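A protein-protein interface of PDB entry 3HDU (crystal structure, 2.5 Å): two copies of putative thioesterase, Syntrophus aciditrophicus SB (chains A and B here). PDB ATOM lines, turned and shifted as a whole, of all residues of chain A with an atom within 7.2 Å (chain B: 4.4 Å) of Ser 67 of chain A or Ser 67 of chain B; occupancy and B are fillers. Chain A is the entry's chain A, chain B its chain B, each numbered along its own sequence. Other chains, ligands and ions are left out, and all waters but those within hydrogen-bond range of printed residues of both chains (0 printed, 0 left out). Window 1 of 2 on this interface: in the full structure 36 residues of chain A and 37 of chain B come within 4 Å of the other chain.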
ATOM      1  N   LEU A  61      19.372  15.607 -29.634  1.00  0.00           N
ATOM      2  CA  LEU A  61      18.932  16.277 -28.386  1.00  0.00           C
ATOM      3  C   LEU A  61      18.001  15.408 -27.516  1.00  0.00           C
ATOM      4  O   LEU A  61      18.106  15.433 -26.286  1.00  0.00           O
ATOM      5  CB  LEU A  61      18.263  17.624 -28.690  1.00  0.00           C
ATOM      6  CG  LEU A  61      19.178  18.732 -29.218  1.00  0.00           C
ATOM      7  CD1 LEU A  61      18.369  19.894 -29.771  1.00  0.00           C
ATOM      8  CD2 LEU A  61      20.128  19.211 -28.129  1.00  0.00           C
ATOM      9  N   TYR A  62      17.111  14.650 -28.161  1.00  0.00           N
ATOM     10  CA  TYR A  62      16.237  13.687 -27.466  1.00  0.00           C
ATOM     11  C   TYR A  62      17.029  12.557 -26.771  1.00  0.00           C
ATOM     12  O   TYR A  62      16.572  12.027 -25.762  1.00  0.00           O
ATOM     13  CB  TYR A  62      15.160  13.107 -28.405  1.00  0.00           C
ATOM     14  CG  TYR A  62      13.916  13.974 -28.559  1.00  0.00           C
ATOM     15  CD1 TYR A  62      13.994  15.278 -29.064  1.00  0.00           C
ATOM     16  CD2 TYR A  62      12.645  13.476 -28.224  1.00  0.00           C
ATOM     17  CE1 TYR A  62      12.839  16.078 -29.215  1.00  0.00           C
ATOM     18  CE2 TYR A  62      11.486  14.262 -28.373  1.00  0.00           C
ATOM     19  CZ  TYR A  62      11.588  15.559 -28.869  1.00  0.00           C
ATOM     20  OH  TYR A  62      10.448  16.325 -29.008  1.00  0.00           O
ATOM     21  N   GLY A  63      18.200  12.197 -27.301  1.00  0.00           N
ATOM     22  CA  GLY A  63      19.078  11.205 -26.670  1.00  0.00           C
ATOM     23  C   GLY A  63      19.491  11.641 -25.273  1.00  0.00           C
ATOM     24  O   GLY A  63      19.400  10.857 -24.322  1.00  0.00           O
ATOM     25  N   GLY A  64      19.920  12.903 -25.163  1.00  0.00           N
ATOM     26  CA  GLY A  64      20.298  13.519 -23.886  1.00  0.00           C
ATOM     27  C   GLY A  64      19.128  13.653 -22.918  1.00  0.00           C
ATOM     28  O   GLY A  64      19.293  13.421 -21.715  1.00  0.00           O
ATOM     29  N   VAL A  65      17.955  14.031 -23.447  1.00  0.00           N
ATOM     30  CA  VAL A  65      16.713  14.145 -22.664  1.00  0.00           C
ATOM     31  C   VAL A  65      16.311  12.784 -22.083  1.00  0.00           C
ATOM     32  O   VAL A  65      16.010  12.695 -20.887  1.00  0.00           O
ATOM     33  CB  VAL A  65      15.538  14.745 -23.510  1.00  0.00           C
ATOM     34  CG1 VAL A  65      14.206  14.645 -22.780  1.00  0.00           C
ATOM     35  CG2 VAL A  65      15.826  16.195 -23.870  1.00  0.00           C
ATOM     36  N   ILE A  66      16.317  11.746 -22.928  1.00  0.00           N
ATOM     37  CA  ILE A  66      15.993  10.363 -22.518  1.00  0.00           C
ATOM     38  C   ILE A  66      16.956   9.838 -21.439  1.00  0.00           C
ATOM     39  O   ILE A  66      16.504   9.202 -20.474  1.00  0.00           O
ATOM     40  CB  ILE A  66      15.968   9.398 -23.741  1.00  0.00           C
ATOM     41  CG1 ILE A  66      14.741   9.675 -24.611  1.00  0.00           C
ATOM     42  CG2 ILE A  66      15.934   7.916 -23.318  1.00  0.00           C
ATOM     43  CD1 ILE A  66      14.814   9.009 -25.976  1.00  0.00           C
ATOM     44  N   SER A  67      18.258  10.113 -21.603  1.00  0.00           N
ATOM     45  CA  SER A  67      19.280   9.699 -20.629  1.00  0.00           C
ATOM     46  C   SER A  67      19.086  10.404 -19.280  1.00  0.00           C
ATOM     47  O   SER A  67      19.263   9.770 -18.240  1.00  0.00           O
ATOM     48  CB  SER A  67      20.713   9.911 -21.159  1.00  0.00           C
ATOM     49  OG  SER A  67      21.028  11.280 -21.373  1.00  0.00           O
ATOM     50  N   SER A  68      18.711  11.691 -19.302  1.00  0.00           N
ATOM     51  CA  SER A  68      18.418  12.451 -18.067  1.00  0.00           C
ATOM     52  C   SER A  68      17.179  11.918 -17.345  1.00  0.00           C
ATOM     53  O   SER A  68      17.221  11.726 -16.133  1.00  0.00           O
ATOM     54  CB  SER A  68      18.227  13.936 -18.350  1.00  0.00           C
ATOM     55  OG  SER A  68      19.436  14.507 -18.801  1.00  0.00           O
ATOM     56  N   ALA A  69      16.096  11.680 -18.095  1.00  0.00           N
ATOM     57  CA  ALA A  69      14.841  11.135 -17.547  1.00  0.00           C
ATOM     58  C   ALA A  69      15.045   9.779 -16.859  1.00  0.00           C
ATOM     59  O   ALA A  69      14.506   9.550 -15.774  1.00  0.00           O
ATOM     60  CB  ALA A  69      13.782  11.010 -18.638  1.00  0.00           C
ATOM     61  N   ILE A  70      15.815   8.897 -17.504  1.00  0.00           N
ATOM     62  CA  ILE A  70      16.166   7.574 -16.952  1.00  0.00           C
ATOM     63  C   ILE A  70      16.999   7.725 -15.664  1.00  0.00           C
ATOM     64  O   ILE A  70      16.726   7.045 -14.671  1.00  0.00           O
ATOM     65  CB  ILE A  70      16.893   6.678 -18.019  1.00  0.00           C
ATOM     66  CG1 ILE A  70      15.882   6.223 -19.082  1.00  0.00           C
ATOM     67  CG2 ILE A  70      17.555   5.454 -17.382  1.00  0.00           C
ATOM     68  CD1 ILE A  70      16.482   5.469 -20.258  1.00  0.00           C
ATOM     69  N   ASP A  71      17.981   8.630 -15.694  1.00  0.00           N
ATOM     70  CA  ASP A  71      18.840   8.921 -14.542  1.00  0.00           C
ATOM     71  C   ASP A  71      18.048   9.488 -13.357  1.00  0.00           C
ATOM     72  O   ASP A  71      18.329   9.139 -12.205  1.00  0.00           O
ATOM     73  CB  ASP A  71      19.963   9.900 -14.936  1.00  0.00           C
ATOM     74  CG  ASP A  71      21.026  10.059 -13.848  1.00  0.00           C
ATOM     75  OD1 ASP A  71      21.387   9.059 -13.196  1.00  0.00           O
ATOM     76  OD2 ASP A  71      21.522  11.187 -13.657  1.00  0.00           O
ATOM     77  N   MET A  72      17.086  10.370 -13.645  1.00  0.00           N
ATOM     78  CA  MET A  72      16.214  10.962 -12.618  1.00  0.00           C
ATOM     79  C   MET A  72      15.266   9.928 -12.013  1.00  0.00           C
ATOM     80  O   MET A  72      15.085   9.908 -10.793  1.00  0.00           O
ATOM     81  CB  MET A  72      15.403  12.137 -13.184  1.00  0.00           C
ATOM     82  CG  MET A  72      16.232  13.375 -13.512  1.00  0.00           C
ATOM     83  SD  MET A  72      17.014  14.219 -11.949  1.00  0.00           S
ATOM     84  CE  MET A  72      15.401  14.653 -10.983  1.00  0.00           C
ATOM     85  N   THR A  73      14.657   9.099 -12.869  1.00  0.00           N
ATOM     86  CA  THR A  73      13.763   8.016 -12.437  1.00  0.00           C
ATOM     87  C   THR A  73      14.530   7.032 -11.552  1.00  0.00           C
ATOM     88  O   THR A  73      14.037   6.640 -10.488  1.00  0.00           O
ATOM     89  CB  THR A  73      13.119   7.266 -13.641  1.00  0.00           C
ATOM     90  OG1 THR A  73      12.408   8.195 -14.464  1.00  0.00           O
ATOM     91  CG2 THR A  73      12.153   6.178 -13.176  1.00  0.00           C
ATOM     92  N   LEU A 106      25.649   4.675 -15.720  1.00  0.00           N
ATOM     93  CA  LEU A 106      24.415   4.881 -16.494  1.00  0.00           C
ATOM     94  C   LEU A 106      24.563   4.188 -17.853  1.00  0.00           C
ATOM     95  O   LEU A 106      25.377   4.617 -18.680  1.00  0.00           O
ATOM     96  CB  LEU A 106      24.153   6.375 -16.702  1.00  0.00           C
ATOM     97  CG  LEU A 106      22.975   6.795 -17.593  1.00  0.00           C
ATOM     98  CD1 LEU A 106      21.654   6.266 -17.045  1.00  0.00           C
ATOM     99  CD2 LEU A 106      22.918   8.301 -17.711  1.00  0.00           C
ATOM    100  N   VAL A 108      22.264   3.047 -21.081  1.00  0.00           N
ATOM    101  CA  VAL A 108      20.976   3.254 -21.758  1.00  0.00           C
ATOM    102  C   VAL A 108      21.031   2.700 -23.184  1.00  0.00           C
ATOM    103  O   VAL A 108      21.921   3.080 -23.939  1.00  0.00           O
ATOM    104  CB  VAL A 108      20.598   4.769 -21.810  1.00  0.00           C
ATOM    105  CG1 VAL A 108      19.278   4.992 -22.564  1.00  0.00           C
ATOM    106  CG2 VAL A 108      20.506   5.347 -20.404  1.00  0.00           C
ATOM    107  N   TYR A 110      18.756   2.349 -26.651  1.00  0.00           N
ATOM    108  CA  TYR A 110      17.640   2.991 -27.362  1.00  0.00           C
ATOM    109  C   TYR A 110      17.105   2.105 -28.490  1.00  0.00           C
ATOM    110  O   TYR A 110      17.863   1.719 -29.386  1.00  0.00           O
ATOM    111  CB  TYR A 110      18.117   4.312 -27.977  1.00  0.00           C
ATOM    112  CG  TYR A 110      18.683   5.344 -27.007  1.00  0.00           C
ATOM    113  CD1 TYR A 110      19.961   5.189 -26.440  1.00  0.00           C
ATOM    114  CD2 TYR A 110      17.971   6.516 -26.702  1.00  0.00           C
ATOM    115  CE1 TYR A 110      20.495   6.149 -25.566  1.00  0.00           C
ATOM    116  CE2 TYR A 110      18.499   7.486 -25.842  1.00  0.00           C
ATOM    117  CZ  TYR A 110      19.762   7.295 -25.273  1.00  0.00           C
ATOM    118  OH  TYR A 110      20.301   8.228 -24.421  1.00  0.00           O
ATOM    119  N   LEU A 139      11.571   3.139 -20.455  1.00  0.00           N
ATOM    120  CA  LEU A 139      11.031   4.419 -20.886  1.00  0.00           C
ATOM    121  C   LEU A 139      10.151   4.205 -22.117  1.00  0.00           C
ATOM    122  O   LEU A 139      10.599   3.594 -23.099  1.00  0.00           O
ATOM    123  CB  LEU A 139      12.159   5.409 -21.160  1.00  0.00           C
ATOM    124  CG  LEU A 139      11.732   6.875 -21.360  1.00  0.00           C
ATOM    125  CD1 LEU A 139      12.794   7.852 -20.863  1.00  0.00           C
ATOM    126  CD2 LEU A 139      11.373   7.156 -22.802  1.00  0.00           C
ATOM    127  N   ALA A 148      13.238   3.132 -24.944  1.00  0.00           N
ATOM    128  CA  ALA A 148      14.561   2.933 -24.330  1.00  0.00           C
ATOM    129  C   ALA A 148      14.496   2.149 -23.015  1.00  0.00           C
ATOM    130  O   ALA A 148      13.469   2.158 -22.336  1.00  0.00           O
ATOM    131  CB  ALA A 148      15.262   4.273 -24.113  1.00  0.00           C
ATOM    132  N   VAL A 152      20.921   1.572 -14.213  1.00  0.00           N
ATOM    133  CA  VAL A 152      21.560   2.677 -13.506  1.00  0.00           C
ATOM    134  C   VAL A 152      21.971   2.248 -12.095  1.00  0.00           C
ATOM    135  O   VAL A 152      21.182   1.613 -11.394  1.00  0.00           O
ATOM    136  CB  VAL A 152      20.606   3.893 -13.404  1.00  0.00           C
ATOM    137  CG1 VAL A 152      21.337   5.114 -12.828  1.00  0.00           C
ATOM    138  CG2 VAL A 152      20.005   4.235 -14.769  1.00  0.00           C
ATOM    139  N   GLY B  63      24.208  14.407 -12.781  1.00  0.00           N
ATOM    140  CA  GLY B  63      24.336  13.120 -13.475  1.00  0.00           C
ATOM    141  C   GLY B  63      23.720  13.153 -14.864  1.00  0.00           C
ATOM    142  O   GLY B  63      24.343  12.707 -15.838  1.00  0.00           O
ATOM    143  N   GLY B  64      22.502  13.695 -14.947  1.00  0.00           N
ATOM    144  CA  GLY B  64      21.783  13.861 -16.215  1.00  0.00           C
ATOM    145  C   GLY B  64      22.439  14.863 -17.156  1.00  0.00           C
ATOM    146  O   GLY B  64      22.463  14.639 -18.367  1.00  0.00           O
ATOM    147  N   VAL B  65      22.964  15.962 -16.602  1.00  0.00           N
ATOM    148  CA  VAL B  65      23.670  16.994 -17.388  1.00  0.00           C
ATOM    149  C   VAL B  65      24.936  16.414 -18.041  1.00  0.00           C
ATOM    150  O   VAL B  65      25.202  16.682 -19.210  1.00  0.00           O
ATOM    151  CB  VAL B  65      24.010  18.256 -16.523  1.00  0.00           C
ATOM    152  CG1 VAL B  65      24.890  19.243 -17.281  1.00  0.00           C
ATOM    153  CG2 VAL B  65      22.736  18.953 -16.065  1.00  0.00           C
ATOM    154  N   ILE B  66      25.690  15.621 -17.277  1.00  0.00           N
ATOM    155  CA  ILE B  66      26.913  14.952 -17.746  1.00  0.00           C
ATOM    156  C   ILE B  66      26.621  13.924 -18.854  1.00  0.00           C
ATOM    157  O   ILE B  66      27.366  13.867 -19.831  1.00  0.00           O
ATOM    158  CB  ILE B  66      27.687  14.295 -16.552  1.00  0.00           C
ATOM    159  CG1 ILE B  66      28.308  15.380 -15.661  1.00  0.00           C
ATOM    160  CG2 ILE B  66      28.805  13.347 -17.034  1.00  0.00           C
ATOM    161  CD1 ILE B  66      28.797  14.874 -14.301  1.00  0.00           C
ATOM    162  N   SER B  67      25.555  13.130 -18.697  1.00  0.00           N
ATOM    163  CA  SER B  67      25.156  12.133 -19.713  1.00  0.00           C
ATOM    164  C   SER B  67      24.761  12.806 -21.035  1.00  0.00           C
ATOM    165  O   SER B  67      25.117  12.307 -22.106  1.00  0.00           O
ATOM    166  CB  SER B  67      24.003  11.241 -19.223  1.00  0.00           C
ATOM    167  OG  SER B  67      22.771  11.949 -19.168  1.00  0.00           O
ATOM    168  N   SER B  68      24.019  13.917 -20.940  1.00  0.00           N
ATOM    169  CA  SER B  68      23.616  14.720 -22.108  1.00  0.00           C
ATOM    170  C   SER B  68      24.817  15.349 -22.795  1.00  0.00           C
ATOM    171  O   SER B  68      24.871  15.368 -24.022  1.00  0.00           O
ATOM    172  CB  SER B  68      22.638  15.833 -21.726  1.00  0.00           C
ATOM    173  OG  SER B  68      21.417  15.291 -21.281  1.00  0.00           O
ATOM    174  N   ALA B  69      25.752  15.879 -21.999  1.00  0.00           N
ATOM    175  CA  ALA B  69      26.995  16.483 -22.514  1.00  0.00           C
ATOM    176  C   ALA B  69      27.810  15.450 -23.296  1.00  0.00           C
ATOM    177  O   ALA B  69      28.274  15.737 -24.406  1.00  0.00           O
ATOM    178  CB  ALA B  69      27.829  17.066 -21.374  1.00  0.00           C
ATOM    179  N   ILE B  70      27.957  14.258 -22.706  1.00  0.00           N
ATOM    180  CA  ILE B  70      28.657  13.113 -23.315  1.00  0.00           C
ATOM    181  C   ILE B  70      27.976  12.682 -24.621  1.00  0.00           C
ATOM    182  O   ILE B  70      28.649  12.529 -25.640  1.00  0.00           O
ATOM    183  CB  ILE B  70      28.785  11.922 -22.305  1.00  0.00           C
ATOM    184  CG1 ILE B  70      29.834  12.266 -21.237  1.00  0.00           C
ATOM    185  CG2 ILE B  70      29.199  10.632 -22.996  1.00  0.00           C
ATOM    186  CD1 ILE B  70      29.927  11.279 -20.088  1.00  0.00           C
ATOM    187  N   ASP B  71      26.652  12.516 -24.575  1.00  0.00           N
ATOM    188  CA  ASP B  71      25.842  12.140 -25.746  1.00  0.00           C
ATOM    189  C   ASP B  71      25.951  13.164 -26.886  1.00  0.00           C
ATOM    190  O   ASP B  71      26.030  12.778 -28.050  1.00  0.00           O
ATOM    191  CB  ASP B  71      24.368  11.955 -25.357  1.00  0.00           C
ATOM    192  CG  ASP B  71      23.517  11.396 -26.492  1.00  0.00           C
ATOM    193  OD1 ASP B  71      23.951  10.443 -27.171  1.00  0.00           O
ATOM    194  OD2 ASP B  71      22.402  11.905 -26.699  1.00  0.00           O
ATOM    195  N   LEU B 106      24.274   4.264 -24.903  1.00  0.00           N
ATOM    196  CA  LEU B 106      25.002   5.272 -24.115  1.00  0.00           C
ATOM    197  C   LEU B 106      25.404   4.639 -22.782  1.00  0.00           C
ATOM    198  O   LEU B 106      24.529   4.296 -21.977  1.00  0.00           O
ATOM    199  CB  LEU B 106      24.126   6.510 -23.876  1.00  0.00           C
ATOM    200  CG  LEU B 106      24.693   7.679 -23.053  1.00  0.00           C
ATOM    201  CD1 LEU B 106      25.891   8.293 -23.723  1.00  0.00           C
ATOM    202  CD2 LEU B 106      23.642   8.737 -22.859  1.00  0.00           C
ATOM    203  N   TYR B 110      30.846   7.178 -13.930  1.00  0.00           N
ATOM    204  CA  TYR B 110      31.200   8.391 -13.175  1.00  0.00           C
ATOM    205  C   TYR B 110      32.285   8.099 -12.122  1.00  0.00           C
ATOM    206  O   TYR B 110      32.109   7.220 -11.281  1.00  0.00           O
ATOM    207  CB  TYR B 110      29.953   8.953 -12.483  1.00  0.00           C
ATOM    208  CG  TYR B 110      28.796   9.307 -13.410  1.00  0.00           C
ATOM    209  CD1 TYR B 110      27.917   8.316 -13.887  1.00  0.00           C
ATOM    210  CD2 TYR B 110      28.549  10.629 -13.784  1.00  0.00           C
ATOM    211  CE1 TYR B 110      26.841   8.629 -14.733  1.00  0.00           C
ATOM    212  CE2 TYR B 110      27.464  10.957 -14.631  1.00  0.00           C
ATOM    213  CZ  TYR B 110      26.615   9.951 -15.100  1.00  0.00           C
ATOM    214  OH  TYR B 110      25.555  10.243 -15.931  1.00  0.00           O
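Among the printed residues, merely in contact across the chains: Gly 63 of chain A with Asp 71 of chain B (3.3 Å), Ser 67 of chain A with Leu 106 of chain B (3.6 Å), Asp 71 of chain A with Gly 63 of chain B (3.2 Å), Leu 106 of chain A with Ser 67 of chain B (3.5 Å), Leu 106 of chain A with Tyr 110 of chain B (3.7 Å) and Tyr 110 of chain A with Leu 106 of chain B (3.7 Å).
The backbone carbonyl oxygen (O) of Gly 63 of chain A lies within hydrogen-bond range of the side-chain hydroxyl (OH) of Tyr 110 of chain A (2.8 Å). O of Gly 64 of chain A is in hydrogen-bond range of OG of Ser 67 of chain A, 2.8 Å away. OG of Ser 68 of chain A sits at hydrogen-bond distance from O of Gly 64 of chain A, at 3.1 Å. The backbone carbonyl oxygen (O) of Gly 63 of chain B lies within hydrogen-bond range of the side-chain hydroxyl (OH) of Tyr 110 of chain B (2.7 Å). The backbone carbonyl oxygen of Gly 64 of chain B sits at hydrogen-bond distance from the side-chain hydroxyl of Ser 67 of chain B. The backbone carbonyl oxygen of Gly 64 of chain B lies within hydrogen-bond range of the side-chain hydroxyl of Ser 68 of chain B.
Of the 19 printed residues of chain A, 8 touch a printed residue of chain B. Printed residues of chain A that touch a printed residue of chain B: Gly 63, Gly 64, Ser 67, Ser 68, Asp 71, Leu 106, Val 108 and Tyr 110. Of the 11 printed residues of chain B, 7 touch a printed residue of chain A. Hydrophobic or aromatic side chains of chain B within 4 Å of the printed part of chain A: Leu 106 and Tyr 110. Along chain B the printed residues that touch a printed residue of chain A span positions 63 to 110. Among the printed residues, 14 pairs touch across the chains. Among the printed residues, no Asp or Glu carboxylate lies within 4 Å of a Lys or Arg side-chain nitrogen of the other chain.
O of Gly 64 of chain A lies within hydrogen-bond range of OG of Ser 68 of chain B (2.9 Å). OD2 of Asp 71 of chain B sits at hydrogen-bond distance from N of Gly 64 of chain A (3.1 Å). The side-chain hydroxyl (OG) of Ser 67 of chain B sits at hydrogen-bond distance from the side-chain hydroxyl (OG) of Ser 67 of chain A, 2.9 Å away. O of Gly 64 of chain B sits at hydrogen-bond distance from OG of Ser 68 of chain A (3.1 Å). OG of Ser 68 of chain A is in hydrogen-bond range of OG of Ser 68 of chain B (3.3 Å). The side-chain carboxylate of Asp 71 of chain A sits at hydrogen-bond distance from the backbone NH of Gly 64 of chain B (3.0 Å). The backbone NH (N) of Val 108 of chain A sits at hydrogen-bond distance from the backbone carbonyl oxygen (O) of Leu 106 of chain B (2.7 Å). The backbone carbonyl oxygen (O) of Leu 106 of chain A lies close to the backbone carbonyl oxygen (O) of Leu 106 of chain B.
Gly 64 of chain A touches Asp 71 of chain B, and with the chains exchanged Asp 71 of chain A touches Gly 64 of chain B. Ser 67 of chain B touches its own counterpart, Ser 67 of chain A. Ser 68 of chain A touches its own counterpart, Ser 68 of chain B. Leu 106 of chain B touches its own counterpart, Leu 106 of chain A. 11 positions are printed for both chains. Of the 14 pairs that touch across the chains among the printed residues, 13 have their exchanged pair printed and touching as well.
Printed residues of chain B within 4 Å of Ser 67 of chain A: Ser 67 (2.9 Å) and Leu 106 (3.6 Å). Ser 67 of chain B touches just these residues of chain A: Ser 67 and Leu 106. Printed residues of chain A within 4 Å of Tyr 110 of chain B: Leu 106. Of the printed residues of chain B, Tyr 110 of chain A touches Leu 106. Of the printed residues of chain B, Ser 68 of chain A touches Gly 64 and Ser 68. Of the printed residues of chain B, Asp 71 of chain A touches Gly 63 (3.2 Å) and Gly 64 (3.0 Å). Printed residues of chain B within 4 Å of Leu 106 of chain A: Ser 67, Leu 106 and Tyr 110. Val 65 of chain A touches none of the printed residues of chain B.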
